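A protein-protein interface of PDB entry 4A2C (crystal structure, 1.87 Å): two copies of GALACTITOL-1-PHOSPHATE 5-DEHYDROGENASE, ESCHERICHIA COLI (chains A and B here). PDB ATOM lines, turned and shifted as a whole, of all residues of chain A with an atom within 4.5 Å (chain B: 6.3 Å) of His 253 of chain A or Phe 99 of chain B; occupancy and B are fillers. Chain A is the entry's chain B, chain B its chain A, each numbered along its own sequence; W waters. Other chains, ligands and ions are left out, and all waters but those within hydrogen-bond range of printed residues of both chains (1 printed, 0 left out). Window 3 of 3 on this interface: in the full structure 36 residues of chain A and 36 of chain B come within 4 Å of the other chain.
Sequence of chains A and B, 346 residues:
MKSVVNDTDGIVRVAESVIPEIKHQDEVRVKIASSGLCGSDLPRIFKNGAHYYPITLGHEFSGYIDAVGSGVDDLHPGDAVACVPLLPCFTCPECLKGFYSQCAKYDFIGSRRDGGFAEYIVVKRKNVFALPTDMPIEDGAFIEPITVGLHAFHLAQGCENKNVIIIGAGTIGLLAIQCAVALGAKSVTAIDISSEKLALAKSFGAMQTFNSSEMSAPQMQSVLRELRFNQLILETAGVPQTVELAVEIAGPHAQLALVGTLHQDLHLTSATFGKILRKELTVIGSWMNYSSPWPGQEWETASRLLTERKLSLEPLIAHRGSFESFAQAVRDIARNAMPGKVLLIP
OE1 of Gln 102 of chain B is in hydrogen-bond range of NE2 of His 253 of chain A.
The side-chain amide nitrogen (NE2) of Gln 102 of chain B is in hydrogen-bond range of the side-chain carboxylate (OE1) of Glu 280 of chain A (3.4 Å).
OE2 of Glu 280 of chain A sits close to NE2 of His 151 of chain B, at 2.3 Å.
The backbone NH (N) of Glu 94 of chain B lies close to the side-chain sulfur (SG) of Cys 92 of chain B (3.7 Å).
The backbone carbonyl oxygen of Lys 279 of chain A lies within hydrogen-bond range of the backbone NH of His 253 of chain A (2.7 Å).
NE2 of His 253 of chain A lies within hydrogen-bond range of OE1 of Glu 280 of chain A, at 2.8 Å.
O of Glu 94 of chain B sits at hydrogen-bond distance from N of Phe 99 of chain B (2.7 Å).
Phe 229 of chain A touches Pro 93 of chain B.
Phe 229 of chain A touches Glu 94 of chain B (CZ to CD, 3.6 Å).
Phe 229 of chain A touches Lys 97 of chain B (CD1 to CD, 3.7 Å).
CE1 of Phe 229 of chain A touches CD2 of Phe 99 of chain B, 3.7 Å away.
His 253 of chain A touches Phe 99 of chain B.
C of Lys 279 of chain A touches NE2 of Gln 102 of chain B (3.8 Å).
OE2 of Glu 280 of chain A touches CD1 of Leu 155 of chain B, at 3.5 Å.
His 253 of chain A touches just these residues of chain B: Phe 99 (3.4 Å) and Gln 102 (3.0 Å).
Phe 99 of chain B touches two residues of chain A.
Of the printed residues of chain B, Lys 279 of chain A touches Gln 102.
Of the printed residues of chain A, His 151 of chain B touches Glu 280.
Of the printed residues of chain B, Glu 280 of chain A touches Gln 102, His 151 and Leu 155.
Of the printed residues of chain A, Leu 155 of chain B touches Glu 280.
Pro 252 of chain A touches none of the printed residues of chain B.
Ser 101 of chain B touches none of the printed residues of chain A.
The nearest residue of chain B that does not touch His 253 of chain A is Leu 155 of chain B (4.5 Å).
The nearest printed residue of chain A that does not touch His 151 of chain B is His 253 of chain A (6.1 Å).
Of the 15 printed residues of chain B, 7 touch a printed residue of chain A.
Printed residues of chain B that touch a printed residue of chain A: Pro 93, Glu 94, Lys 97, Phe 99, Gln 102, His 151 and Leu 155.
Of the 8 printed residues of chain A, 4 touch a printed residue of chain B.
Hydrophobic or aromatic side chains of chain A that line the printed part of chain B: Phe 229 and His 253.
Among the printed residues, 10 pairs touch across the chains.
No position is printed for both chains.
Water W1 lies within hydrogen-bond range of the side-chain carboxylate (OE1) of Glu 280 of chain A (2.4 Å) and a ring nitrogen (NE2) of His 151 of chain B (3.3 Å).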
ATOM      1  N   PHE A 229      -4.496  -9.366  16.178  1.00  0.00           N
ATOM      2  CA  PHE A 229      -3.358  -8.548  15.757  1.00  0.00           C
ATOM      3  C   PHE A 229      -2.966  -7.492  16.788  1.00  0.00           C
ATOM      4  O   PHE A 229      -3.802  -7.069  17.598  1.00  0.00           O
ATOM      5  CB  PHE A 229      -3.652  -7.894  14.407  1.00  0.00           C
ATOM      6  CG  PHE A 229      -3.763  -8.887  13.256  1.00  0.00           C
ATOM      7  CD1 PHE A 229      -2.625  -9.433  12.672  1.00  0.00           C
ATOM      8  CD2 PHE A 229      -5.000  -9.278  12.778  1.00  0.00           C
ATOM      9  CE1 PHE A 229      -2.732 -10.351  11.606  1.00  0.00           C
ATOM     10  CE2 PHE A 229      -5.112 -10.186  11.717  1.00  0.00           C
ATOM     11  CZ  PHE A 229      -3.976 -10.719  11.137  1.00  0.00           C
ATOM     12  N   GLY A 251      -1.938 -14.193  19.538  1.00  0.00           N
ATOM     13  CA  GLY A 251      -2.198 -13.947  18.129  1.00  0.00           C
ATOM     14  C   GLY A 251      -0.896 -13.722  17.349  1.00  0.00           C
ATOM     15  O   GLY A 251       0.188 -13.649  17.932  1.00  0.00           O
ATOM     16  N   PRO A 252      -0.999 -13.588  16.016  1.00  0.00           N
ATOM     17  CA  PRO A 252       0.190 -13.484  15.156  1.00  0.00           C
ATOM     18  C   PRO A 252       1.061 -12.303  15.554  1.00  0.00           C
ATOM     19  O   PRO A 252       0.549 -11.168  15.679  1.00  0.00           O
ATOM     20  CB  PRO A 252      -0.397 -13.270  13.742  1.00  0.00           C
ATOM     21  CG  PRO A 252      -1.831 -12.824  13.981  1.00  0.00           C
ATOM     22  CD  PRO A 252      -2.259 -13.492  15.255  1.00  0.00           C
ATOM     23  N   HIS A 253       2.357 -12.568  15.744  1.00  0.00           N
ATOM     24  CA  HIS A 253       3.304 -11.528  16.135  1.00  0.00           C
ATOM     25  C   HIS A 253       2.941 -10.790  17.439  1.00  0.00           C
ATOM     26  O   HIS A 253       3.294  -9.622  17.615  1.00  0.00           O
ATOM     27  CB  HIS A 253       3.509 -10.531  14.990  1.00  0.00           C
ATOM     28  CG  HIS A 253       4.289 -11.094  13.834  1.00  0.00           C
ATOM     29  ND1 HIS A 253       5.533 -10.611  13.478  1.00  0.00           N
ATOM     30  CD2 HIS A 253       4.019 -12.103  12.975  1.00  0.00           C
ATOM     31  CE1 HIS A 253       5.989 -11.291  12.443  1.00  0.00           C
ATOM     32  NE2 HIS A 253       5.094 -12.200  12.112  1.00  0.00           N
ATOM     33  N   ALA A 254       2.267 -11.467  18.360  1.00  0.00           N
ATOM     34  CA  ALA A 254       1.956 -10.823  19.642  1.00  0.00           C
ATOM     35  C   ALA A 254       3.228 -10.521  20.442  1.00  0.00           C
ATOM     36  O   ALA A 254       4.241 -11.205  20.298  1.00  0.00           O
ATOM     37  CB  ALA A 254       1.009 -11.675  20.456  1.00  0.00           C
ATOM     38  N   GLN A 255       3.167  -9.466  21.250  1.00  0.00           N
ATOM     39  CA  GLN A 255       4.205  -9.164  22.241  1.00  0.00           C
ATOM     40  C   GLN A 255       3.788  -9.730  23.587  1.00  0.00           C
ATOM     41  O   GLN A 255       2.699  -9.438  24.068  1.00  0.00           O
ATOM     42  CB  GLN A 255       4.372  -7.658  22.370  1.00  0.00           C
ATOM     43  CG  GLN A 255       4.904  -6.969  21.131  1.00  0.00           C
ATOM     44  CD  GLN A 255       4.981  -5.472  21.332  1.00  0.00           C
ATOM     45  OE1 GLN A 255       3.954  -4.795  21.484  1.00  0.00           O
ATOM     46  NE2 GLN A 255       6.201  -4.948  21.375  1.00  0.00           N
ATOM     47  N   LYS A 279       4.192 -18.376  15.611  1.00  0.00           N
ATOM     48  CA  LYS A 279       3.435 -17.137  15.638  1.00  0.00           C
ATOM     49  C   LYS A 279       4.371 -15.935  15.532  1.00  0.00           C
ATOM     50  O   LYS A 279       3.914 -14.780  15.502  1.00  0.00           O
ATOM     51  CB  LYS A 279       2.602 -17.056  16.917  1.00  0.00           C
ATOM     52  CG  LYS A 279       1.625 -18.215  17.106  1.00  0.00           C
ATOM     53  CD  LYS A 279       0.896 -18.097  18.463  1.00  0.00           C
ATOM     54  CE  LYS A 279      -0.132 -19.199  18.659  1.00  0.00           C
ATOM     55  NZ  LYS A 279      -0.946 -18.989  19.901  1.00  0.00           N
ATOM     56  N   GLU A 280       5.675 -16.220  15.457  1.00  0.00           N
ATOM     57  CA  GLU A 280       6.723 -15.195  15.561  1.00  0.00           C
ATOM     58  C   GLU A 280       6.454 -14.211  16.731  1.00  0.00           C
ATOM     59  O   GLU A 280       6.451 -12.981  16.590  1.00  0.00           O
ATOM     60  CB  GLU A 280       6.969 -14.496  14.215  1.00  0.00           C
ATOM     61  CG  GLU A 280       7.720 -15.405  13.187  1.00  0.00           C
ATOM     62  CD  GLU A 280       7.979 -14.738  11.851  1.00  0.00           C
ATOM     63  OE1 GLU A 280       7.122 -13.953  11.382  1.00  0.00           O
ATOM     64  OE2 GLU A 280       9.040 -15.003  11.242  1.00  0.00           O
ATOM     65  N   CYS B  92      -5.505 -12.894   2.896  1.00  0.00           N
ATOM     66  CA  CYS B  92      -6.080 -12.968   4.244  1.00  0.00           C
ATOM     67  C   CYS B  92      -5.473 -11.864   5.118  1.00  0.00           C
ATOM     68  O   CYS B  92      -4.503 -11.219   4.706  1.00  0.00           O
ATOM     69  CB  CYS B  92      -5.805 -14.346   4.849  1.00  0.00           C
ATOM     70  SG  CYS B  92      -4.065 -14.634   5.311  1.00  0.00           S
ATOM     71  N   PRO B  93      -6.036 -11.627   6.321  1.00  0.00           N
ATOM     72  CA  PRO B  93      -5.461 -10.500   7.065  1.00  0.00           C
ATOM     73  C   PRO B  93      -3.966 -10.683   7.356  1.00  0.00           C
ATOM     74  O   PRO B  93      -3.206  -9.719   7.195  1.00  0.00           O
ATOM     75  CB  PRO B  93      -6.311 -10.450   8.361  1.00  0.00           C
ATOM     76  CG  PRO B  93      -7.624 -11.110   7.970  1.00  0.00           C
ATOM     77  CD  PRO B  93      -7.199 -12.215   7.014  1.00  0.00           C
ATOM     78  N   GLU B  94      -3.537 -11.875   7.767  1.00  0.00           N
ATOM     79  CA  GLU B  94      -2.111 -12.118   7.969  1.00  0.00           C
ATOM     80  C   GLU B  94      -1.250 -11.736   6.753  1.00  0.00           C
ATOM     81  O   GLU B  94      -0.268 -11.003   6.903  1.00  0.00           O
ATOM     82  CB  GLU B  94      -1.830 -13.565   8.404  1.00  0.00           C
ATOM     83  CG  GLU B  94      -2.216 -13.870   9.812  1.00  0.00           C
ATOM     84  CD  GLU B  94      -3.700 -14.104   9.986  1.00  0.00           C
ATOM     85  OE1 GLU B  94      -4.487 -13.810   9.058  1.00  0.00           O
ATOM     86  OE2 GLU B  94      -4.086 -14.585  11.064  1.00  0.00           O
ATOM     87  N   CYS B  95      -1.613 -12.202   5.559  1.00  0.00           N
ATOM     88  CA  CYS B  95      -0.865 -11.853   4.350  1.00  0.00           C
ATOM     89  C   CYS B  95      -0.883 -10.359   4.029  1.00  0.00           C
ATOM     90  O   CYS B  95       0.136  -9.802   3.627  1.00  0.00           O
ATOM     91  CB  CYS B  95      -1.374 -12.656   3.140  1.00  0.00           C
ATOM     92  SG  CYS B  95      -1.003 -14.446   3.253  1.00  0.00           S
ATOM     93  N   LEU B  96      -2.030  -9.706   4.210  1.00  0.00           N
ATOM     94  CA  LEU B  96      -2.119  -8.289   3.871  1.00  0.00           C
ATOM     95  C   LEU B  96      -1.148  -7.483   4.726  1.00  0.00           C
ATOM     96  O   LEU B  96      -0.613  -6.469   4.281  1.00  0.00           O
ATOM     97  CB  LEU B  96      -3.547  -7.756   4.036  1.00  0.00           C
ATOM     98  CG  LEU B  96      -4.604  -8.231   3.029  1.00  0.00           C
ATOM     99  CD1 LEU B  96      -5.955  -7.667   3.427  1.00  0.00           C
ATOM    100  CD2 LEU B  96      -4.253  -7.838   1.588  1.00  0.00           C
ATOM    101  N   LYS B  97      -0.914  -7.948   5.949  1.00  0.00           N
ATOM    102  CA  LYS B  97       0.017  -7.265   6.845  1.00  0.00           C
ATOM    103  C   LYS B  97       1.458  -7.763   6.695  1.00  0.00           C
ATOM    104  O   LYS B  97       2.369  -7.251   7.349  1.00  0.00           O
ATOM    105  CB  LYS B  97      -0.453  -7.376   8.293  1.00  0.00           C
ATOM    106  CG  LYS B  97      -1.692  -6.545   8.616  1.00  0.00           C
ATOM    107  CD  LYS B  97      -2.181  -6.872  10.020  1.00  0.00           C
ATOM    108  CE  LYS B  97      -3.586  -6.317  10.278  1.00  0.00           C
ATOM    109  NZ  LYS B  97      -3.592  -4.834  10.409  1.00  0.00           N
ATOM    110  N   GLY B  98       1.675  -8.756   5.836  1.00  0.00           N
ATOM    111  CA  GLY B  98       3.026  -9.226   5.562  1.00  0.00           C
ATOM    112  C   GLY B  98       3.429 -10.423   6.406  1.00  0.00           C
ATOM    113  O   GLY B  98       4.593 -10.836   6.399  1.00  0.00           O
ATOM    114  N   PHE B  99       2.465 -10.965   7.147  1.00  0.00           N
ATOM    115  CA  PHE B  99       2.697 -12.124   7.996  1.00  0.00           C
ATOM    116  C   PHE B  99       2.470 -13.420   7.203  1.00  0.00           C
ATOM    117  O   PHE B  99       1.706 -14.288   7.632  1.00  0.00           O
ATOM    118  CB  PHE B  99       1.768 -12.076   9.228  1.00  0.00           C
ATOM    119  CG  PHE B  99       1.964 -10.861  10.126  1.00  0.00           C
ATOM    120  CD1 PHE B  99       3.170 -10.156  10.150  1.00  0.00           C
ATOM    121  CD2 PHE B  99       0.944 -10.454  10.980  1.00  0.00           C
ATOM    122  CE1 PHE B  99       3.348  -9.057  10.996  1.00  0.00           C
ATOM    123  CE2 PHE B  99       1.110  -9.354  11.835  1.00  0.00           C
ATOM    124  CZ  PHE B  99       2.309  -8.651  11.842  1.00  0.00           C
ATOM    125  N   TYR B 100       3.130 -13.553   6.047  1.00  0.00           N
ATOM    126  CA  TYR B 100       2.873 -14.693   5.157  1.00  0.00           C
ATOM    127  C   TYR B 100       3.101 -16.046   5.845  1.00  0.00           C
ATOM    128  O   TYR B 100       2.427 -17.032   5.532  1.00  0.00           O
ATOM    129  CB  TYR B 100       3.731 -14.621   3.880  1.00  0.00           C
ATOM    130  CG  TYR B 100       3.772 -13.261   3.208  1.00  0.00           C
ATOM    131  CD1 TYR B 100       2.683 -12.767   2.503  1.00  0.00           C
ATOM    132  CD2 TYR B 100       4.925 -12.482   3.258  1.00  0.00           C
ATOM    133  CE1 TYR B 100       2.736 -11.509   1.876  1.00  0.00           C
ATOM    134  CE2 TYR B 100       4.988 -11.246   2.642  1.00  0.00           C
ATOM    135  CZ  TYR B 100       3.901 -10.761   1.960  1.00  0.00           C
ATOM    136  OH  TYR B 100       3.987  -9.523   1.355  1.00  0.00           O
ATOM    137  N   SER B 101       4.038 -16.078   6.786  1.00  0.00           N
ATOM    138  CA  SER B 101       4.409 -17.313   7.463  1.00  0.00           C
ATOM    139  C   SER B 101       3.439 -17.659   8.591  1.00  0.00           C
ATOM    140  O   SER B 101       3.629 -18.664   9.271  1.00  0.00           O
ATOM    141  CB  SER B 101       5.836 -17.225   8.001  1.00  0.00           C
ATOM    142  OG  SER B 101       6.729 -16.934   6.942  1.00  0.00           O
ATOM    143  N   GLN B 102       2.421 -16.817   8.786  1.00  0.00           N
ATOM    144  CA  GLN B 102       1.310 -17.130   9.683  1.00  0.00           C
ATOM    145  C   GLN B 102       0.032 -17.286   8.870  1.00  0.00           C
ATOM    146  O   GLN B 102      -1.075 -17.240   9.417  1.00  0.00           O
ATOM    147  CB  GLN B 102       1.098 -16.045  10.749  1.00  0.00           C
ATOM    148  CG  GLN B 102       2.139 -16.051  11.876  1.00  0.00           C
ATOM    149  CD  GLN B 102       3.453 -15.446  11.439  1.00  0.00           C
ATOM    150  OE1 GLN B 102       3.473 -14.392  10.792  1.00  0.00           O
ATOM    151  NE2 GLN B 102       4.564 -16.115  11.771  1.00  0.00           N
ATOM    152  N   CYS B 103       0.173 -17.446   7.561  1.00  0.00           N
ATOM    153  CA  CYS B 103      -1.002 -17.722   6.744  1.00  0.00           C
ATOM    154  C   CYS B 103      -1.435 -19.158   7.020  1.00  0.00           C
ATOM    155  O   CYS B 103      -0.595 -20.062   7.027  1.00  0.00           O
ATOM    156  CB  CYS B 103      -0.698 -17.509   5.259  1.00  0.00           C
ATOM    157  SG  CYS B 103      -2.076 -17.873   4.109  1.00  0.00           S
ATOM    158  N   HIS B 151      16.248 -13.818   7.945  1.00  0.00           N
ATOM    159  CA  HIS B 151      14.920 -13.481   8.442  1.00  0.00           C
ATOM    160  C   HIS B 151      14.982 -13.283   9.951  1.00  0.00           C
ATOM    161  O   HIS B 151      14.293 -12.429  10.498  1.00  0.00           O
ATOM    162  CB  HIS B 151      13.863 -14.533   8.073  1.00  0.00           C
ATOM    163  CG  HIS B 151      12.518 -14.269   8.678  1.00  0.00           C
ATOM    164  ND1 HIS B 151      11.732 -13.196   8.314  1.00  0.00           N
ATOM    165  CD2 HIS B 151      11.827 -14.928   9.641  1.00  0.00           C
ATOM    166  CE1 HIS B 151      10.610 -13.210   9.017  1.00  0.00           C
ATOM    167  NE2 HIS B 151      10.645 -14.252   9.831  1.00  0.00           N
ATOM    168  N   LEU B 155      14.045  -9.796  11.847  1.00  0.00           N
ATOM    169  CA  LEU B 155      13.167  -9.702  13.026  1.00  0.00           C
ATOM    170  C   LEU B 155      13.829  -8.986  14.192  1.00  0.00           C
ATOM    171  O   LEU B 155      13.151  -8.363  15.020  1.00  0.00           O
ATOM    172  CB  LEU B 155      12.721 -11.086  13.467  1.00  0.00           C
ATOM    173  CG  LEU B 155      11.765 -11.759  12.482  1.00  0.00           C
ATOM    174  CD1 LEU B 155      11.490 -13.193  12.923  1.00  0.00           C
ATOM    175  CD2 LEU B 155      10.469 -10.952  12.374  1.00  0.00           C
ATOM    176  N   SER B 292       7.559  -8.512   3.914  1.00  0.00           N
ATOM    177  CA  SER B 292       6.879  -7.722   2.894  1.00  0.00           C
ATOM    178  C   SER B 292       7.783  -6.644   2.309  1.00  0.00           C
ATOM    179  O   SER B 292       8.584  -6.045   3.027  1.00  0.00           O
ATOM    180  CB  SER B 292       5.623  -7.071   3.475  1.00  0.00           C
ATOM    181  OG  SER B 292       5.977  -6.213   4.539  1.00  0.00           O
HETATM  182  O   HOH W   1       7.583 -13.173   9.147  1.00  0.00           O
